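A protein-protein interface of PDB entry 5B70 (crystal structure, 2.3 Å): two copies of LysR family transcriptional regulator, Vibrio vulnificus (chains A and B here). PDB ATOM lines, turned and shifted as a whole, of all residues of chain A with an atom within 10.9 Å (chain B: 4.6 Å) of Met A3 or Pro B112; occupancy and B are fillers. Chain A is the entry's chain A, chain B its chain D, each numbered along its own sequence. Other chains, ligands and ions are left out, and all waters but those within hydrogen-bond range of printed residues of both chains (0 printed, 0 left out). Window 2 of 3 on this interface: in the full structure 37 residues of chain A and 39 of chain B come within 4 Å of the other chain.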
ATOM      1  N   GLY A   1       0.486  21.957 -10.535  1.00  0.00           N
ATOM      2  CA  GLY A   1       0.072  22.047  -9.146  1.00  0.00           C
ATOM      3  C   GLY A   1       1.177  21.790  -8.134  1.00  0.00           C
ATOM      4  O   GLY A   1       2.253  21.302  -8.486  1.00  0.00           O
ATOM      5  N   ALA A   2       0.908  22.118  -6.870  1.00  0.00           N
ATOM      6  CA  ALA A   2       1.878  21.944  -5.796  1.00  0.00           C
ATOM      7  C   ALA A   2       1.133  21.713  -4.486  1.00  0.00           C
ATOM      8  O   ALA A   2      -0.101  21.746  -4.432  1.00  0.00           O
ATOM      9  CB  ALA A   2       2.815  23.152  -5.696  1.00  0.00           C
ATOM     10  N   MET A   3       1.896  21.485  -3.421  1.00  0.00           N
ATOM     11  CA  MET A   3       1.320  21.235  -2.103  1.00  0.00           C
ATOM     12  C   MET A   3       1.000  22.537  -1.378  1.00  0.00           C
ATOM     13  O   MET A   3      -0.119  22.734  -0.903  1.00  0.00           O
ATOM     14  CB  MET A   3       2.271  20.388  -1.262  1.00  0.00           C
ATOM     15  CG  MET A   3       2.636  19.062  -1.898  1.00  0.00           C
ATOM     16  SD  MET A   3       3.884  18.168  -0.958  1.00  0.00           S
ATOM     17  CE  MET A   3       5.214  19.365  -0.934  1.00  0.00           C
ATOM     18  N   GLY A  16      -6.202  27.276  -7.298  1.00  0.00           N
ATOM     19  CA  GLY A  16      -6.801  26.728  -6.095  1.00  0.00           C
ATOM     20  C   GLY A  16      -6.933  25.214  -6.171  1.00  0.00           C
ATOM     21  O   GLY A  16      -5.965  24.513  -6.468  1.00  0.00           O
ATOM     22  N   GLN A  17      -8.138  24.713  -5.902  1.00  0.00           N
ATOM     23  CA  GLN A  17      -8.387  23.285  -5.830  1.00  0.00           C
ATOM     24  C   GLN A  17      -9.614  22.930  -6.659  1.00  0.00           C
ATOM     25  O   GLN A  17     -10.517  23.750  -6.853  1.00  0.00           O
ATOM     26  CB  GLN A  17      -8.586  22.825  -4.380  1.00  0.00           C
ATOM     27  CG  GLN A  17      -8.371  21.338  -4.158  1.00  0.00           C
ATOM     28  CD  GLN A  17      -8.782  20.895  -2.769  1.00  0.00           C
ATOM     29  OE1 GLN A  17      -8.023  20.222  -2.070  1.00  0.00           O
ATOM     30  NE2 GLN A  17      -9.991  21.270  -2.363  1.00  0.00           N
ATOM     31  N   ASN A  39      -0.175  20.974 -15.257  1.00  0.00           N
ATOM     32  CA  ASN A  39       0.992  21.364 -14.467  1.00  0.00           C
ATOM     33  C   ASN A  39       1.775  22.495 -15.121  1.00  0.00           C
ATOM     34  O   ASN A  39       2.391  23.307 -14.420  1.00  0.00           O
ATOM     35  CB  ASN A  39       1.905  20.159 -14.239  1.00  0.00           C
ATOM     36  CG  ASN A  39       1.319  19.159 -13.264  1.00  0.00           C
ATOM     37  OD1 ASN A  39       0.498  19.508 -12.416  1.00  0.00           O
ATOM     38  ND2 ASN A  39       1.743  17.905 -13.376  1.00  0.00           N
ATOM     39  N   PRO A  43      -0.071  26.512 -13.541  1.00  0.00           N
ATOM     40  CA  PRO A  43       0.845  25.909 -12.563  1.00  0.00           C
ATOM     41  C   PRO A  43       0.266  25.731 -11.166  1.00  0.00           C
ATOM     42  O   PRO A  43       0.887  25.024 -10.363  1.00  0.00           O
ATOM     43  CB  PRO A  43       2.030  26.895 -12.538  1.00  0.00           C
ATOM     44  CG  PRO A  43       1.634  28.068 -13.375  1.00  0.00           C
ATOM     45  CD  PRO A  43       0.553  27.614 -14.290  1.00  0.00           C
ATOM     46  N   GLN A  44      -0.879  26.333 -10.837  1.00  0.00           N
ATOM     47  CA  GLN A  44      -1.394  26.301  -9.469  1.00  0.00           C
ATOM     48  C   GLN A  44      -2.836  25.822  -9.425  1.00  0.00           C
ATOM     49  O   GLN A  44      -3.652  26.326  -8.648  1.00  0.00           O
ATOM     50  CB  GLN A  44      -1.265  27.672  -8.808  1.00  0.00           C
ATOM     51  CG  GLN A  44       0.165  28.183  -8.726  1.00  0.00           C
ATOM     52  CD  GLN A  44       0.549  28.636  -7.329  1.00  0.00           C
ATOM     53  OE1 GLN A  44       1.276  27.939  -6.620  1.00  0.00           O
ATOM     54  NE2 GLN A  44       0.073  29.810  -6.932  1.00  0.00           N
ATOM     55  N   LEU A  45      -3.169  24.823 -10.237  1.00  0.00           N
ATOM     56  CA  LEU A  45      -4.465  24.160 -10.177  1.00  0.00           C
ATOM     57  C   LEU A  45      -4.245  22.750  -9.646  1.00  0.00           C
ATOM     58  O   LEU A  45      -3.707  21.890 -10.354  1.00  0.00           O
ATOM     59  CB  LEU A  45      -5.147  24.138 -11.542  1.00  0.00           C
ATOM     60  CG  LEU A  45      -6.525  23.476 -11.536  1.00  0.00           C
ATOM     61  CD1 LEU A  45      -7.434  24.137 -10.509  1.00  0.00           C
ATOM     62  CD2 LEU A  45      -7.151  23.535 -12.912  1.00  0.00           C
ATOM     63  N   ASN A  46      -4.643  22.523  -8.396  1.00  0.00           N
ATOM     64  CA  ASN A  46      -4.541  21.216  -7.761  1.00  0.00           C
ATOM     65  C   ASN A  46      -5.798  20.408  -8.057  1.00  0.00           C
ATOM     66  O   ASN A  46      -6.918  20.895  -7.868  1.00  0.00           O
ATOM     67  CB  ASN A  46      -4.337  21.368  -6.253  1.00  0.00           C
ATOM     68  CG  ASN A  46      -2.991  21.988  -5.905  1.00  0.00           C
ATOM     69  OD1 ASN A  46      -2.324  22.571  -6.758  1.00  0.00           O
ATOM     70  ND2 ASN A  46      -2.586  21.854  -4.644  1.00  0.00           N
ATOM     71  N   LEU A  47      -5.610  19.174  -8.522  1.00  0.00           N
ATOM     72  CA  LEU A  47      -6.705  18.333  -8.992  1.00  0.00           C
ATOM     73  C   LEU A  47      -6.777  17.066  -8.151  1.00  0.00           C
ATOM     74  O   LEU A  47      -5.843  16.257  -8.159  1.00  0.00           O
ATOM     75  CB  LEU A  47      -6.521  17.987 -10.471  1.00  0.00           C
ATOM     76  CG  LEU A  47      -7.795  17.900 -11.309  1.00  0.00           C
ATOM     77  CD1 LEU A  47      -8.551  19.219 -11.253  1.00  0.00           C
ATOM     78  CD2 LEU A  47      -7.467  17.530 -12.745  1.00  0.00           C
ATOM     79  N   LEU A  48      -7.880  16.895  -7.428  1.00  0.00           N
ATOM     80  CA  LEU A  48      -8.148  15.670  -6.690  1.00  0.00           C
ATOM     81  C   LEU A  48      -9.030  14.762  -7.535  1.00  0.00           C
ATOM     82  O   LEU A  48      -9.994  15.221  -8.158  1.00  0.00           O
ATOM     83  CB  LEU A  48      -8.819  15.966  -5.347  1.00  0.00           C
ATOM     84  CG  LEU A  48      -7.977  16.762  -4.346  1.00  0.00           C
ATOM     85  CD1 LEU A  48      -8.781  17.062  -3.095  1.00  0.00           C
ATOM     86  CD2 LEU A  48      -6.690  16.020  -3.995  1.00  0.00           C
ATOM     87  N   GLN B  98       8.278  19.199  -7.058  1.00  0.00           N
ATOM     88  CA  GLN B  98       8.556  19.151  -5.630  1.00  0.00           C
ATOM     89  C   GLN B  98       9.780  18.305  -5.303  1.00  0.00           C
ATOM     90  O   GLN B  98       9.928  17.854  -4.161  1.00  0.00           O
ATOM     91  CB  GLN B  98       7.334  18.633  -4.867  1.00  0.00           C
ATOM     92  CG  GLN B  98       6.322  19.711  -4.500  1.00  0.00           C
ATOM     93  CD  GLN B  98       5.807  20.468  -5.708  1.00  0.00           C
ATOM     94  OE1 GLN B  98       5.370  19.868  -6.689  1.00  0.00           O
ATOM     95  NE2 GLN B  98       5.865  21.794  -5.645  1.00  0.00           N
ATOM     96  N   ILE B 102      11.328  18.564  -1.255  1.00  0.00           N
ATOM     97  CA  ILE B 102      11.462  17.408  -0.376  1.00  0.00           C
ATOM     98  C   ILE B 102      12.847  16.811  -0.578  1.00  0.00           C
ATOM     99  O   ILE B 102      13.254  16.550  -1.715  1.00  0.00           O
ATOM    100  CB  ILE B 102      10.376  16.349  -0.644  1.00  0.00           C
ATOM    101  CG1 ILE B 102       8.994  16.883  -0.261  1.00  0.00           C
ATOM    102  CG2 ILE B 102      10.694  15.074   0.111  1.00  0.00           C
ATOM    103  CD1 ILE B 102       8.243  17.530  -1.399  1.00  0.00           C
ATOM    104  N   ASP B 110       9.697  15.828   8.374  1.00  0.00           N
ATOM    105  CA  ASP B 110      10.041  17.065   7.685  1.00  0.00           C
ATOM    106  C   ASP B 110       9.053  17.424   6.582  1.00  0.00           C
ATOM    107  O   ASP B 110       9.099  18.549   6.074  1.00  0.00           O
ATOM    108  CB  ASP B 110      11.454  16.962   7.106  1.00  0.00           C
ATOM    109  CG  ASP B 110      12.161  18.300   7.053  1.00  0.00           C
ATOM    110  OD1 ASP B 110      12.732  18.713   8.085  1.00  0.00           O
ATOM    111  OD2 ASP B 110      12.150  18.941   5.980  1.00  0.00           O
ATOM    112  N   LEU B 111       8.159  16.505   6.208  1.00  0.00           N
ATOM    113  CA  LEU B 111       7.185  16.752   5.158  1.00  0.00           C
ATOM    114  C   LEU B 111       6.072  17.671   5.649  1.00  0.00           C
ATOM    115  O   LEU B 111       5.748  17.685   6.839  1.00  0.00           O
ATOM    116  CB  LEU B 111       6.569  15.443   4.681  1.00  0.00           C
ATOM    117  CG  LEU B 111       7.453  14.487   3.890  1.00  0.00           C
ATOM    118  CD1 LEU B 111       6.823  13.109   3.854  1.00  0.00           C
ATOM    119  CD2 LEU B 111       7.646  15.021   2.487  1.00  0.00           C
ATOM    120  N   PRO B 112       5.473  18.451   4.751  1.00  0.00           N
ATOM    121  CA  PRO B 112       4.197  19.091   5.079  1.00  0.00           C
ATOM    122  C   PRO B 112       3.113  18.039   5.209  1.00  0.00           C
ATOM    123  O   PRO B 112       3.176  16.970   4.597  1.00  0.00           O
ATOM    124  CB  PRO B 112       3.939  20.017   3.886  1.00  0.00           C
ATOM    125  CG  PRO B 112       4.698  19.398   2.769  1.00  0.00           C
ATOM    126  CD  PRO B 112       5.924  18.788   3.390  1.00  0.00           C
ATOM    127  N   ASP B 113       2.117  18.343   6.029  1.00  0.00           N
ATOM    128  CA  ASP B 113       1.112  17.356   6.381  1.00  0.00           C
ATOM    129  C   ASP B 113      -0.146  17.556   5.549  1.00  0.00           C
ATOM    130  O   ASP B 113      -0.383  18.630   4.987  1.00  0.00           O
ATOM    131  CB  ASP B 113       0.801  17.416   7.876  1.00  0.00           C
ATOM    132  CG  ASP B 113       2.055  17.536   8.712  1.00  0.00           C
ATOM    133  OD1 ASP B 113       1.961  17.853   9.915  1.00  0.00           O
ATOM    134  OD2 ASP B 113       3.151  17.388   8.134  1.00  0.00           O
ATOM    135  N   GLU B 114      -0.954  16.494   5.485  1.00  0.00           N
ATOM    136  CA  GLU B 114      -1.988  16.333   4.461  1.00  0.00           C
ATOM    137  C   GLU B 114      -1.356  16.279   3.070  1.00  0.00           C
ATOM    138  O   GLU B 114      -1.898  16.803   2.094  1.00  0.00           O
ATOM    139  CB  GLU B 114      -3.057  17.427   4.545  1.00  0.00           C
ATOM    140  CG  GLU B 114      -3.955  17.320   5.767  1.00  0.00           C
ATOM    141  CD  GLU B 114      -5.143  18.266   5.705  1.00  0.00           C
ATOM    142  OE1 GLU B 114      -5.544  18.784   6.769  1.00  0.00           O
ATOM    143  OE2 GLU B 114      -5.677  18.488   4.596  1.00  0.00           O
ATOM    144  N   SER B 115      -0.193  15.630   2.985  1.00  0.00           N
ATOM    145  CA  SER B 115       0.535  15.456   1.736  1.00  0.00           C
ATOM    146  C   SER B 115       0.680  14.005   1.309  1.00  0.00           C
ATOM    147  O   SER B 115       0.790  13.741   0.110  1.00  0.00           O
ATOM    148  CB  SER B 115       1.938  16.077   1.840  1.00  0.00           C
ATOM    149  OG  SER B 115       2.716  15.423   2.830  1.00  0.00           O
ATOM    150  N   GLY B 159       1.736  16.918  -8.295  1.00  0.00           N
ATOM    151  CA  GLY B 159       2.549  17.556  -7.281  1.00  0.00           C
ATOM    152  C   GLY B 159       1.865  17.807  -5.957  1.00  0.00           C
ATOM    153  O   GLY B 159       2.322  18.667  -5.196  1.00  0.00           O
ATOM    154  N   LEU B 160       0.786  17.084  -5.651  1.00  0.00           N
ATOM    155  CA  LEU B 160       0.036  17.318  -4.423  1.00  0.00           C
ATOM    156  C   LEU B 160       0.627  16.598  -3.222  1.00  0.00           C
ATOM    157  O   LEU B 160       0.134  16.785  -2.105  1.00  0.00           O
ATOM    158  CB  LEU B 160      -1.424  16.895  -4.597  1.00  0.00           C
ATOM    159  CG  LEU B 160      -2.133  17.357  -5.871  1.00  0.00           C
ATOM    160  CD1 LEU B 160      -3.629  17.104  -5.764  1.00  0.00           C
ATOM    161  CD2 LEU B 160      -1.848  18.821  -6.144  1.00  0.00           C
ATOM    162  N   GLY B 161       1.653  15.796  -3.420  1.00  0.00           N
ATOM    163  CA  GLY B 161       2.302  15.111  -2.332  1.00  0.00           C
ATOM    164  C   GLY B 161       3.035  13.878  -2.850  1.00  0.00           C
ATOM    165  O   GLY B 161       3.621  13.905  -3.936  1.00  0.00           O
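N of Met A3 sits close to O of Gly B159.
N of Gly A1 is in hydrogen-bond range of OD1 of Asn A39, at 3.1 Å.
The backbone NH (N) of Gly A1 sits at hydrogen-bond distance from the backbone carbonyl oxygen (O) of Pro A43, 3.1 Å away.
The backbone carbonyl oxygen of Ala A2 lies within hydrogen-bond range of the side-chain amide nitrogen of Asn A46.
O of Gly A16 sits at hydrogen-bond distance from N of Asn A46 (3.1 Å).
OE1 of Gln B98 touches O of Gly A1, at 3.9 Å.
Gly B159 touches Gly A1 (CA to O, 3.9 Å).
Ala A2 touches Gln B98.
Ala A2 touches Gly B159.
CE of Met A3 touches CG of Gln B98 (3.8 Å).
Ser B115 touches Met A3 (CB to SD, 3.998 Å).
Leu B160 touches Met A3.
CG of Asn A46 touches CD2 of Leu B160, at 3.4 Å.
CD1 of Leu B160 touches O of Leu A47 (3.4 Å).
CD2 of Leu A48 touches CD1 of Leu B160 (3.7 Å).
Of the printed residues of chain B, Met A3 touches Gln B98, Ile B102, Pro B112, Ser B115, Gly B159, Leu B160 and Gly B161.
Of chain A, only Met A3 (3.7 Å) comes within 4 Å of Pro B112.
No residue of chain A comes within 4 Å of Leu B111.
No residue of chain A comes within 4 Å of Asp B113.
Of chain A, only Gly A1, Ala A2 and Met A3 come within 4 Å of Gly B159.
Of chain A, only Met A3 (3.7 Å) comes within 4 Å of Gly B161.
Printed residues of chain B within 4 Å of Gly A1: Gln B98 and Gly B159.
Of the printed residues of chain B, Leu A48 touches Leu B160 (3.7 Å).
Printed residues of chain A within 4 Å of Leu B160: Ala A2 (3.8 Å), Met A3 (3.4 Å), Asn A46 (3.4 Å), Leu A47 (3.4 Å) and Leu A48 (3.7 Å).
Of the printed residues of chain B, Ala A2 touches Gln B98, Gly B159 and Leu B160.
Leu A45 touches none of the printed residues of chain B.
The nearest printed residue of chain B that does not touch Met A3 is Leu B111 (6.0 Å).
The nearest residue of chain A that does not touch Pro B112 is Ala A2 (8.4 Å).
The nearest printed residue of chain B that does not touch Asn A46 is Gly B159 (5.9 Å).
Of the 12 printed residues of chain A, 6 touch a printed residue of chain B.
Along chain A the printed residues that touch a printed residue of chain B span positions 1 to 48.
Among the printed residues, 15 pairs touch across the chains.
No position is printed for both chains.
Of the 15 pairs that touch across the chains among the printed residues, none has its exchanged pair printed and touching as well.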
